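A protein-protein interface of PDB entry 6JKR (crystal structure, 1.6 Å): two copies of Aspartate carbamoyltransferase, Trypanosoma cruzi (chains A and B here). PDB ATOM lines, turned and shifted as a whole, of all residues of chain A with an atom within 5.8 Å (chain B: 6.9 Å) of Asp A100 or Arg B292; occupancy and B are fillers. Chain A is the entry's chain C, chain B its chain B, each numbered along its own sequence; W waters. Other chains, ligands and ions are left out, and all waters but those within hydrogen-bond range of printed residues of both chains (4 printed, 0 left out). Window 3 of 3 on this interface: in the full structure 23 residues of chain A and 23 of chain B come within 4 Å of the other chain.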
ATOM      1  N   LYS A  94      11.701   4.806 -13.366  1.00  0.00           N
ATOM      2  CA  LYS A  94      12.385   3.535 -13.614  1.00  0.00           C
ATOM      3  C   LYS A  94      11.381   2.452 -14.023  1.00  0.00           C
ATOM      4  O   LYS A  94      11.690   1.262 -13.992  1.00  0.00           O
ATOM      5  CB  LYS A  94      13.183   3.108 -12.383  1.00  0.00           C
ATOM      6  CG  LYS A  94      14.418   3.990 -12.125  1.00  0.00           C
ATOM      7  CD  LYS A  94      15.137   3.651 -10.821  1.00  0.00           C
ATOM      8  CE  LYS A  94      16.418   4.478 -10.671  1.00  0.00           C
ATOM      9  NZ  LYS A  94      16.854   4.568  -9.231  1.00  0.00           N
ATOM     10  N   GLY A  95      10.173   2.875 -14.379  1.00  0.00           N
ATOM     11  CA  GLY A  95       9.157   1.942 -14.830  1.00  0.00           C
ATOM     12  C   GLY A  95       8.252   1.389 -13.752  1.00  0.00           C
ATOM     13  O   GLY A  95       7.486   0.458 -14.022  1.00  0.00           O
ATOM     14  N   GLU A  96       8.296   1.956 -12.544  1.00  0.00           N
ATOM     15  CA  GLU A  96       7.423   1.463 -11.489  1.00  0.00           C
ATOM     16  C   GLU A  96       5.968   1.736 -11.834  1.00  0.00           C
ATOM     17  O   GLU A  96       5.615   2.857 -12.212  1.00  0.00           O
ATOM     18  CB  GLU A  96       7.768   2.083 -10.122  1.00  0.00           C
ATOM     19  CG  GLU A  96       7.031   1.419  -8.960  1.00  0.00           C
ATOM     20  CD  GLU A  96       7.763   1.515  -7.621  1.00  0.00           C
ATOM     21  OE1 GLU A  96       7.701   0.535  -6.850  1.00  0.00           O
ATOM     22  OE2 GLU A  96       8.380   2.567  -7.347  1.00  0.00           O
ATOM     23  N   THR A  97       5.121   0.724 -11.659  1.00  0.00           N
ATOM     24  CA  THR A  97       3.702   0.835 -11.983  1.00  0.00           C
ATOM     25  C   THR A  97       2.939   1.646 -10.924  1.00  0.00           C
ATOM     26  O   THR A  97       3.410   1.859  -9.791  1.00  0.00           O
ATOM     27  CB  THR A  97       2.996  -0.539 -12.057  1.00  0.00           C
ATOM     28  OG1 THR A  97       3.226  -1.223 -10.820  1.00  0.00           O
ATOM     29  CG2 THR A  97       3.577  -1.382 -13.182  1.00  0.00           C
ATOM     30  N   LEU A  98       1.765   2.108 -11.303  1.00  0.00           N
ATOM     31  CA  LEU A  98       0.919   2.824 -10.367  1.00  0.00           C
ATOM     32  C   LEU A  98       0.607   1.950  -9.153  1.00  0.00           C
ATOM     33  O   LEU A  98       0.735   2.408  -8.006  1.00  0.00           O
ATOM     34  CB  LEU A  98      -0.380   3.298 -11.051  1.00  0.00           C
ATOM     35  CG  LEU A  98      -1.402   3.906 -10.102  1.00  0.00           C
ATOM     36  CD1 LEU A  98      -0.839   5.229  -9.519  1.00  0.00           C
ATOM     37  CD2 LEU A  98      -2.723   4.141 -10.827  1.00  0.00           C
ATOM     38  N   ALA A  99       0.245   0.692  -9.389  1.00  0.00           N
ATOM     39  CA  ALA A  99      -0.018  -0.251  -8.305  1.00  0.00           C
ATOM     40  C   ALA A  99       1.145  -0.366  -7.341  1.00  0.00           C
ATOM     41  O   ALA A  99       0.942  -0.328  -6.112  1.00  0.00           O
ATOM     42  CB  ALA A  99      -0.388  -1.622  -8.849  1.00  0.00           C
ATOM     43  N   ASP A 100       2.340  -0.560  -7.868  1.00  0.00           N
ATOM     44  CA  ASP A 100       3.487  -0.683  -6.987  1.00  0.00           C
ATOM     45  C   ASP A 100       3.767   0.637  -6.215  1.00  0.00           C
ATOM     46  O   ASP A 100       4.191   0.595  -5.049  1.00  0.00           O
ATOM     47  CB  ASP A 100       4.722  -1.106  -7.780  1.00  0.00           C
ATOM     48  CG  ASP A 100       4.780  -2.614  -8.047  1.00  0.00           C
ATOM     49  OD1 ASP A 100       3.867  -3.364  -7.627  1.00  0.00           O
ATOM     50  OD2 ASP A 100       5.771  -3.024  -8.693  1.00  0.00           O
ATOM     51  N   THR A 101       3.565   1.783  -6.859  1.00  0.00           N
ATOM     52  CA  THR A 101       3.739   3.091  -6.193  1.00  0.00           C
ATOM     53  C   THR A 101       2.762   3.228  -5.024  1.00  0.00           C
ATOM     54  O   THR A 101       3.139   3.646  -3.935  1.00  0.00           O
ATOM     55  CB  THR A 101       3.518   4.243  -7.193  1.00  0.00           C
ATOM     56  OG1 THR A 101       4.543   4.158  -8.184  1.00  0.00           O
ATOM     57  CG2 THR A 101       3.638   5.626  -6.502  1.00  0.00           C
ATOM     58  N   ILE A 102       1.505   2.842  -5.251  1.00  0.00           N
ATOM     59  CA  ILE A 102       0.505   2.859  -4.173  1.00  0.00           C
ATOM     60  C   ILE A 102       0.917   1.942  -3.019  1.00  0.00           C
ATOM     61  O   ILE A 102       0.875   2.340  -1.844  1.00  0.00           O
ATOM     62  CB  ILE A 102      -0.889   2.478  -4.666  1.00  0.00           C
ATOM     63  CG1 ILE A 102      -1.378   3.449  -5.753  1.00  0.00           C
ATOM     64  CG2 ILE A 102      -1.878   2.383  -3.476  1.00  0.00           C
ATOM     65  CD1 ILE A 102      -1.393   4.896  -5.335  1.00  0.00           C
ATOM     66  N   ARG A 103       1.287   0.699  -3.337  1.00  0.00           N
ATOM     67  CA  ARG A 103       1.776  -0.236  -2.320  1.00  0.00           C
ATOM     68  C   ARG A 103       2.953   0.337  -1.522  1.00  0.00           C
ATOM     69  O   ARG A 103       3.046   0.162  -0.308  1.00  0.00           O
ATOM     70  CB  ARG A 103       2.223  -1.536  -2.967  1.00  0.00           C
ATOM     71  CG  ARG A 103       1.109  -2.294  -3.656  1.00  0.00           C
ATOM     72  CD  ARG A 103       1.700  -3.554  -4.204  1.00  0.00           C
ATOM     73  NE  ARG A 103       0.681  -4.487  -4.649  1.00  0.00           N
ATOM     74  CZ  ARG A 103       0.463  -4.790  -5.922  1.00  0.00           C
ATOM     75  NH1 ARG A 103      -0.489  -5.667  -6.214  1.00  0.00           N
ATOM     76  NH2 ARG A 103       1.188  -4.212  -6.893  1.00  0.00           N
ATOM     77  N   THR A 104       3.843   1.032  -2.207  1.00  0.00           N
ATOM     78  CA  THR A 104       5.004   1.641  -1.566  1.00  0.00           C
ATOM     79  C   THR A 104       4.562   2.689  -0.541  1.00  0.00           C
ATOM     80  O   THR A 104       4.894   2.580   0.649  1.00  0.00           O
ATOM     81  CB  THR A 104       5.938   2.276  -2.615  1.00  0.00           C
ATOM     82  OG1 THR A 104       6.380   1.225  -3.496  1.00  0.00           O
ATOM     83  CG2 THR A 104       7.135   2.948  -1.914  1.00  0.00           C
ATOM     84  N   LEU A 105       3.799   3.689  -0.980  1.00  0.00           N
ATOM     85  CA  LEU A 105       3.411   4.747  -0.012  1.00  0.00           C
ATOM     86  C   LEU A 105       2.460   4.216   1.077  1.00  0.00           C
ATOM     87  O   LEU A 105       2.482   4.675   2.218  1.00  0.00           O
ATOM     88  CB  LEU A 105       2.906   6.027  -0.719  1.00  0.00           C
ATOM     89  CG  LEU A 105       4.031   6.921  -1.340  1.00  0.00           C
ATOM     90  CD1 LEU A 105       5.127   7.317  -0.347  1.00  0.00           C
ATOM     91  CD2 LEU A 105       4.685   6.269  -2.529  1.00  0.00           C
ATOM     92  N   ARG B  66      11.162   4.352  -2.303  1.00  0.00           N
ATOM     93  CA  ARG B  66      11.224   3.706  -0.989  1.00  0.00           C
ATOM     94  C   ARG B  66      12.184   4.354  -0.026  1.00  0.00           C
ATOM     95  O   ARG B  66      11.814   4.655   1.123  1.00  0.00           O
ATOM     96  CB  ARG B  66      11.673   2.246  -1.156  1.00  0.00           C
ATOM     97  CG  ARG B  66      10.527   1.298  -1.503  1.00  0.00           C
ATOM     98  CD  ARG B  66      11.074   0.197  -2.468  1.00  0.00           C
ATOM     99  NE  ARG B  66      11.287   0.863  -3.767  1.00  0.00           N
ATOM    100  CZ  ARG B  66      10.324   1.123  -4.650  1.00  0.00           C
ATOM    101  NH1 ARG B  66       9.074   0.674  -4.429  1.00  0.00           N
ATOM    102  NH2 ARG B  66      10.596   1.851  -5.723  1.00  0.00           N
ATOM    103  N   THR B 243      16.548  -8.693  -8.610  1.00  0.00           N
ATOM    104  CA  THR B 243      16.797  -7.275  -8.806  1.00  0.00           C
ATOM    105  C   THR B 243      16.469  -6.911 -10.251  1.00  0.00           C
ATOM    106  O   THR B 243      16.370  -7.806 -11.126  1.00  0.00           O
ATOM    107  CB  THR B 243      18.280  -6.919  -8.535  1.00  0.00           C
ATOM    108  OG1 THR B 243      19.097  -7.708  -9.405  1.00  0.00           O
ATOM    109  CG2 THR B 243      18.693  -7.190  -7.066  1.00  0.00           C
ATOM    110  N   ARG B 244      16.343  -5.605 -10.466  1.00  0.00           N
ATOM    111  CA  ARG B 244      16.059  -4.997 -11.760  1.00  0.00           C
ATOM    112  C   ARG B 244      17.368  -4.657 -12.436  1.00  0.00           C
ATOM    113  O   ARG B 244      18.334  -4.240 -11.779  1.00  0.00           O
ATOM    114  CB  ARG B 244      15.266  -3.695 -11.489  1.00  0.00           C
ATOM    115  CG  ARG B 244      14.816  -2.874 -12.689  1.00  0.00           C
ATOM    116  CD  ARG B 244      14.465  -1.450 -12.212  1.00  0.00           C
ATOM    117  NE  ARG B 244      14.596  -0.479 -13.295  1.00  0.00           N
ATOM    118  CZ  ARG B 244      15.564   0.428 -13.411  1.00  0.00           C
ATOM    119  NH1 ARG B 244      16.504   0.569 -12.484  1.00  0.00           N
ATOM    120  NH2 ARG B 244      15.565   1.234 -14.461  1.00  0.00           N
ATOM    121  N   HIS B 288      12.786  -8.516  -3.187  1.00  0.00           N
ATOM    122  CA  HIS B 288      13.193  -7.640  -4.284  1.00  0.00           C
ATOM    123  C   HIS B 288      13.268  -6.274  -3.621  1.00  0.00           C
ATOM    124  O   HIS B 288      12.301  -5.879  -2.989  1.00  0.00           O
ATOM    125  CB  HIS B 288      12.121  -7.656  -5.392  1.00  0.00           C
ATOM    126  CG  HIS B 288      12.563  -6.995  -6.673  1.00  0.00           C
ATOM    127  ND1 HIS B 288      13.188  -5.769  -6.711  1.00  0.00           N
ATOM    128  CD2 HIS B 288      12.481  -7.409  -7.963  1.00  0.00           C
ATOM    129  CE1 HIS B 288      13.472  -5.450  -7.962  1.00  0.00           C
ATOM    130  NE2 HIS B 288      13.038  -6.427  -8.747  1.00  0.00           N
ATOM    131  N   PRO B 289      14.410  -5.576  -3.712  1.00  0.00           N
ATOM    132  CA  PRO B 289      14.494  -4.229  -3.094  1.00  0.00           C
ATOM    133  C   PRO B 289      13.512  -3.224  -3.692  1.00  0.00           C
ATOM    134  O   PRO B 289      13.144  -2.252  -3.004  1.00  0.00           O
ATOM    135  CB  PRO B 289      15.965  -3.808  -3.343  1.00  0.00           C
ATOM    136  CG  PRO B 289      16.362  -4.600  -4.593  1.00  0.00           C
ATOM    137  CD  PRO B 289      15.624  -5.913  -4.490  1.00  0.00           C
ATOM    138  N   LEU B 290      13.124  -3.456  -4.950  1.00  0.00           N
ATOM    139  CA  LEU B 290      12.217  -2.612  -5.727  1.00  0.00           C
ATOM    140  C   LEU B 290      12.912  -1.279  -6.096  1.00  0.00           C
ATOM    141  O   LEU B 290      13.936  -0.933  -5.492  1.00  0.00           O
ATOM    142  CB  LEU B 290      10.855  -2.431  -5.000  1.00  0.00           C
ATOM    143  CG  LEU B 290      10.108  -3.743  -4.723  1.00  0.00           C
ATOM    144  CD1 LEU B 290       8.864  -3.426  -3.926  1.00  0.00           C
ATOM    145  CD2 LEU B 290       9.748  -4.501  -6.020  1.00  0.00           C
ATOM    146  N   PRO B 291      12.452  -0.602  -7.163  1.00  0.00           N
ATOM    147  CA  PRO B 291      11.354  -0.969  -8.065  1.00  0.00           C
ATOM    148  C   PRO B 291      11.685  -2.176  -8.929  1.00  0.00           C
ATOM    149  O   PRO B 291      12.856  -2.459  -9.180  1.00  0.00           O
ATOM    150  CB  PRO B 291      11.226   0.261  -8.944  1.00  0.00           C
ATOM    151  CG  PRO B 291      12.642   0.815  -9.007  1.00  0.00           C
ATOM    152  CD  PRO B 291      13.137   0.636  -7.603  1.00  0.00           C
ATOM    153  N   ARG B 292      10.630  -2.866  -9.346  1.00  0.00           N
ATOM    154  CA  ARG B 292      10.736  -3.990 -10.261  1.00  0.00           C
ATOM    155  C   ARG B 292      10.246  -3.632 -11.632  1.00  0.00           C
ATOM    156  O   ARG B 292       9.388  -2.745 -11.806  1.00  0.00           O
ATOM    157  CB  ARG B 292       9.935  -5.198  -9.764  1.00  0.00           C
ATOM    158  CG  ARG B 292       8.450  -4.915  -9.657  1.00  0.00           C
ATOM    159  CD  ARG B 292       7.664  -6.151  -9.441  1.00  0.00           C
ATOM    160  NE  ARG B 292       6.311  -5.782  -9.013  1.00  0.00           N
ATOM    161  CZ  ARG B 292       5.354  -6.657  -8.758  1.00  0.00           C
ATOM    162  NH1 ARG B 292       5.559  -7.956  -8.991  1.00  0.00           N
ATOM    163  NH2 ARG B 292       4.185  -6.217  -8.285  1.00  0.00           N
ATOM    164  N   ASN B 293      10.793  -4.370 -12.589  1.00  0.00           N
ATOM    165  CA  ASN B 293      10.240  -4.404 -13.933  1.00  0.00           C
ATOM    166  C   ASN B 293       9.752  -5.840 -14.177  1.00  0.00           C
ATOM    167  O   ASN B 293       9.208  -6.443 -13.262  1.00  0.00           O
ATOM    168  CB  ASN B 293      11.272  -3.863 -14.925  1.00  0.00           C
ATOM    169  CG  ASN B 293      11.572  -2.368 -14.713  1.00  0.00           C
ATOM    170  OD1 ASN B 293      10.788  -1.607 -14.097  1.00  0.00           O
ATOM    171  ND2 ASN B 293      12.705  -1.948 -15.193  1.00  0.00           N
ATOM    172  N   ASP B 294       9.931  -6.381 -15.378  1.00  0.00           N
ATOM    173  CA  ASP B 294       9.323  -7.668 -15.717  1.00  0.00           C
ATOM    174  C   ASP B 294       9.959  -8.902 -15.074  1.00  0.00           C
ATOM    175  O   ASP B 294       9.372 -10.003 -15.141  1.00  0.00           O
ATOM    176  CB  ASP B 294       9.277  -7.832 -17.239  1.00  0.00           C
ATOM    177  CG  ASP B 294       8.437  -6.767 -17.897  1.00  0.00           C
ATOM    178  OD1 ASP B 294       7.586  -6.177 -17.199  1.00  0.00           O
ATOM    179  OD2 ASP B 294       8.628  -6.512 -19.104  1.00  0.00           O
ATOM    180  N   GLU B 295      11.127  -8.729 -14.441  1.00  0.00           N
ATOM    181  CA  GLU B 295      11.862  -9.855 -13.849  1.00  0.00           C
ATOM    182  C   GLU B 295      11.103 -10.536 -12.703  1.00  0.00           C
ATOM    183  O   GLU B 295      11.390 -11.656 -12.312  1.00  0.00           O
ATOM    184  CB  GLU B 295      13.262  -9.422 -13.394  1.00  0.00           C
ATOM    185  CG  GLU B 295      13.307  -8.471 -12.165  1.00  0.00           C
ATOM    186  CD  GLU B 295      12.888  -7.040 -12.459  1.00  0.00           C
ATOM    187  OE1 GLU B 295      12.797  -6.632 -13.658  1.00  0.00           O
ATOM    188  OE2 GLU B 295      12.729  -6.261 -11.493  1.00  0.00           O
ATOM    189  N   LEU B 296      10.127  -9.830 -12.155  1.00  0.00           N
ATOM    190  CA  LEU B 296       9.319 -10.367 -11.074  1.00  0.00           C
ATOM    191  C   LEU B 296       7.863 -10.114 -11.433  1.00  0.00           C
ATOM    192  O   LEU B 296       7.338  -8.986 -11.296  1.00  0.00           O
ATOM    193  CB  LEU B 296       9.694  -9.674  -9.748  1.00  0.00           C
ATOM    194  CG  LEU B 296       8.863 -10.077  -8.530  1.00  0.00           C
ATOM    195  CD1 LEU B 296       8.850 -11.616  -8.332  1.00  0.00           C
ATOM    196  CD2 LEU B 296       9.433  -9.438  -7.278  1.00  0.00           C
ATOM    197  N   SER B 297       7.226 -11.177 -11.901  1.00  0.00           N
ATOM    198  CA  SER B 297       5.877 -11.077 -12.445  1.00  0.00           C
ATOM    199  C   SER B 297       4.832 -10.791 -11.371  1.00  0.00           C
ATOM    200  O   SER B 297       4.941 -11.269 -10.222  1.00  0.00           O
ATOM    201  CB  SER B 297       5.557 -12.381 -13.174  1.00  0.00           C
ATOM    202  OG  SER B 297       4.194 -12.438 -13.534  1.00  0.00           O
ATOM    203  N   THR B 298       3.816 -10.006 -11.750  1.00  0.00           N
ATOM    204  CA  THR B 298       2.711  -9.690 -10.840  1.00  0.00           C
ATOM    205  C   THR B 298       1.928 -10.965 -10.468  1.00  0.00           C
ATOM    206  O   THR B 298       1.169 -10.979  -9.489  1.00  0.00           O
ATOM    207  CB  THR B 298       1.735  -8.644 -11.426  1.00  0.00           C
ATOM    208  OG1 THR B 298       1.244  -9.104 -12.700  1.00  0.00           O
ATOM    209  CG2 THR B 298       2.437  -7.299 -11.615  1.00  0.00           C
ATOM    210  N   THR B 299       2.112 -12.031 -11.242  1.00  0.00           N
ATOM    211  CA  THR B 299       1.505 -13.326 -10.918  1.00  0.00           C
ATOM    212  C   THR B 299       1.992 -13.922  -9.599  1.00  0.00           C
ATOM    213  O   THR B 299       1.387 -14.856  -9.063  1.00  0.00           O
ATOM    214  CB  THR B 299       1.701 -14.388 -12.045  1.00  0.00           C
ATOM    215  OG1 THR B 299       3.092 -14.652 -12.245  1.00  0.00           O
ATOM    216  CG2 THR B 299       1.089 -13.904 -13.367  1.00  0.00           C
ATOM    217  N   VAL B 300       3.103 -13.407  -9.088  1.00  0.00           N
ATOM    218  CA  VAL B 300       3.636 -13.918  -7.844  1.00  0.00           C
ATOM    219  C   VAL B 300       3.053 -13.153  -6.654  1.00  0.00           C
ATOM    220  O   VAL B 300       3.116 -13.620  -5.531  1.00  0.00           O
ATOM    221  CB  VAL B 300       5.180 -13.786  -7.852  1.00  0.00           C
ATOM    222  CG1 VAL B 300       5.824 -14.354  -6.559  1.00  0.00           C
ATOM    223  CG2 VAL B 300       5.745 -14.528  -9.069  1.00  0.00           C
ATOM    224  N   ASP B 301       2.498 -11.972  -6.899  1.00  0.00           N
ATOM    225  CA  ASP B 301       2.125 -11.051  -5.796  1.00  0.00           C
ATOM    226  C   ASP B 301       1.177 -11.629  -4.720  1.00  0.00           C
ATOM    227  O   ASP B 301       1.264 -11.235  -3.549  1.00  0.00           O
ATOM    228  CB  ASP B 301       1.531  -9.750  -6.362  1.00  0.00           C
ATOM    229  CG  ASP B 301       2.505  -8.958  -7.188  1.00  0.00           C
ATOM    230  OD1 ASP B 301       3.692  -9.350  -7.349  1.00  0.00           O
ATOM    231  OD2 ASP B 301       2.049  -7.940  -7.733  1.00  0.00           O
ATOM    232  N   TYR B 308       8.161  -9.141  -0.821  1.00  0.00           N
ATOM    233  CA  TYR B 308       8.733  -7.890  -1.268  1.00  0.00           C
ATOM    234  C   TYR B 308       7.898  -6.656  -0.962  1.00  0.00           C
ATOM    235  O   TYR B 308       8.431  -5.533  -0.974  1.00  0.00           O
ATOM    236  CB  TYR B 308       9.138  -7.937  -2.755  1.00  0.00           C
ATOM    237  CG  TYR B 308       8.170  -8.683  -3.649  1.00  0.00           C
ATOM    238  CD1 TYR B 308       7.130  -8.007  -4.317  1.00  0.00           C
ATOM    239  CD2 TYR B 308       8.291 -10.063  -3.809  1.00  0.00           C
ATOM    240  CE1 TYR B 308       6.248  -8.715  -5.158  1.00  0.00           C
ATOM    241  CE2 TYR B 308       7.416 -10.778  -4.624  1.00  0.00           C
ATOM    242  CZ  TYR B 308       6.422 -10.104  -5.294  1.00  0.00           C
ATOM    243  OH  TYR B 308       5.560 -10.828  -6.091  1.00  0.00           O
ATOM    244  N   PHE B 309       6.611  -6.812  -0.680  1.00  0.00           N
ATOM    245  CA  PHE B 309       5.869  -5.643  -0.182  1.00  0.00           C
ATOM    246  C   PHE B 309       6.066  -5.516   1.320  1.00  0.00           C
ATOM    247  O   PHE B 309       6.296  -4.416   1.816  1.00  0.00           O
ATOM    248  CB  PHE B 309       4.374  -5.716  -0.561  1.00  0.00           C
ATOM    249  CG  PHE B 309       4.152  -5.932  -2.028  1.00  0.00           C
ATOM    250  CD1 PHE B 309       4.774  -5.094  -2.965  1.00  0.00           C
ATOM    251  CD2 PHE B 309       3.322  -6.951  -2.473  1.00  0.00           C
ATOM    252  CE1 PHE B 309       4.586  -5.294  -4.345  1.00  0.00           C
ATOM    253  CE2 PHE B 309       3.111  -7.146  -3.843  1.00  0.00           C
ATOM    254  CZ  PHE B 309       3.736  -6.335  -4.761  1.00  0.00           C
ATOM    255  N   MET B 312       9.189  -3.629   2.387  1.00  0.00           N
ATOM    256  CA  MET B 312       9.181  -2.161   2.458  1.00  0.00           C
ATOM    257  C   MET B 312       8.784  -1.640   3.843  1.00  0.00           C
ATOM    258  O   MET B 312       9.373  -0.664   4.331  1.00  0.00           O
ATOM    259  CB  MET B 312       8.275  -1.573   1.368  1.00  0.00           C
ATOM    260  CG  MET B 312       8.797  -1.780  -0.067  1.00  0.00           C
ATOM    261  SD  MET B 312       7.820  -0.804  -1.236  1.00  0.00           S
ATOM    262  CE  MET B 312       6.349  -1.875  -1.477  1.00  0.00           C
HETATM  263  O   HOH W   1       6.593  -2.013 -11.129  1.00  0.00           O
HETATM  264  O   HOH W   2      -0.426  -7.341  -8.419  1.00  0.00           O
HETATM  265  O   HOH W   3       7.610  -1.993 -15.146  1.00  0.00           O
HETATM  266  O   HOH W   4       8.096  -1.785  -8.109  1.00  0.00           O
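NH1 of Arg B66 lies within salt-bridge range of OE1 of Glu A96 (2.8 Å). OG1 of Thr A104 lies within hydrogen-bond range of NH1 of Arg B66, 2.9 Å away. O of Lys A94 lies within hydrogen-bond range of NE of Arg B244, 3.5 Å away. NE of Arg B292 is in salt-bridge range of OD2 of Asp A100, at 2.8 Å. The side-chain amide oxygen (OD1) of Asn B293 lies close to the backbone carbonyl oxygen (O) of Lys A94, 3.0 Å away. NH1 of Arg A103 lies within salt-bridge range of OD2 of Asp B301 (3.7 Å). SD of Met B312 sits at hydrogen-bond distance from OG1 of Thr A104, at 3.4 Å.
NE of Arg B244 sits close to ND2 of Asn B293. NH1 of Arg B292 sits at hydrogen-bond distance from O of Leu B296. OD2 of Asp B301 lies within salt-bridge range of NH2 of Arg B292. OH of Tyr B308 is in hydrogen-bond range of OD1 of Asp B301, 2.7 Å away. OG1 of Thr A97 is in hydrogen-bond range of N of Asp A100 (3.2 Å). The side-chain carboxylate (OD1) of Asp A100 is in salt-bridge range of the guanidinium group (NH2) of Arg A103 (2.9 Å).
Among the printed residues, pairs that only touch across the chains: Arg A103 with Phe B309 (3.4 Å), Arg A103 with Arg B292 (3.9 Å), Asp A100 with Phe B309 (3.9 Å), Gly A95 with Asn B293 (3.9 Å) and Glu A96 with Pro B291 (3.9 Å).
Printed residues of chain B within 4 Å of Lys A94: Arg B244 and Asn B293. Of chain B, only Arg B292 (2.8 Å) and Phe B309 (3.9 Å) come within 4 Å of Asp A100. Of the printed residues of chain B, Arg A103 touches Arg B292 (3.9 Å), Asp B301 (3.7 Å) and Phe B309 (3.4 Å). His B288 touches none of the printed residues of chain A. Printed residues of chain A within 4 Å of Arg B292: Asp A100 and Arg A103. Glu B295 touches none of the printed residues of chain A. Of the printed residues of chain A, Phe B309 touches Asp A100 (3.9 Å) and Arg A103 (3.4 Å).
Of the 20 printed residues of chain B, 8 touch a printed residue of chain A. Printed residues of chain B that touch a printed residue of chain A: Arg B66, Arg B244, Pro B291, Arg B292, Asn B293, Asp B301, Phe B309 and Met B312. Hydrophobic or aromatic side chains of chain B that line the printed part of chain A: Pro B291, Phe B309 and Met B312. Along chain B the printed residues that touch a printed residue of chain A span positions 66 to 312. Of the 12 printed residues of chain A, 6 touch a printed residue of chain B. Printed residues of chain A that touch a printed residue of chain B: Lys A94, Gly A95, Glu A96, Asp A100, Arg A103 and Thr A104. Among the printed residues, 12 pairs touch across the chains.
No position is printed for both chains. Of the 12 pairs that touch across the chains among the printed residues, none has its exchanged pair printed and touching as well.
Water W2 lies within hydrogen-bond range of OD2 of Asp B301 (2.6 Å) and NH1 of Arg A103 (2.8 Å). Water W4 lies within hydrogen-bond range of the side-chain carboxylate of Glu A96, the side-chain carboxylate of Asp A100 and the backbone NH of Arg B292. Water W3 lies within hydrogen-bond range of the backbone carbonyl oxygen (O) of Gly A95 (2.7 Å) and the side-chain amide oxygen (OD1) of Asn B293 (3.4 Å). Water W1 lies within hydrogen-bond range of the side-chain carboxylate of Asp A100 (2.8 Å), the backbone carbonyl oxygen of Arg B292 (3.0 Å) and the backbone NH of Thr A97 (3.2 Å).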
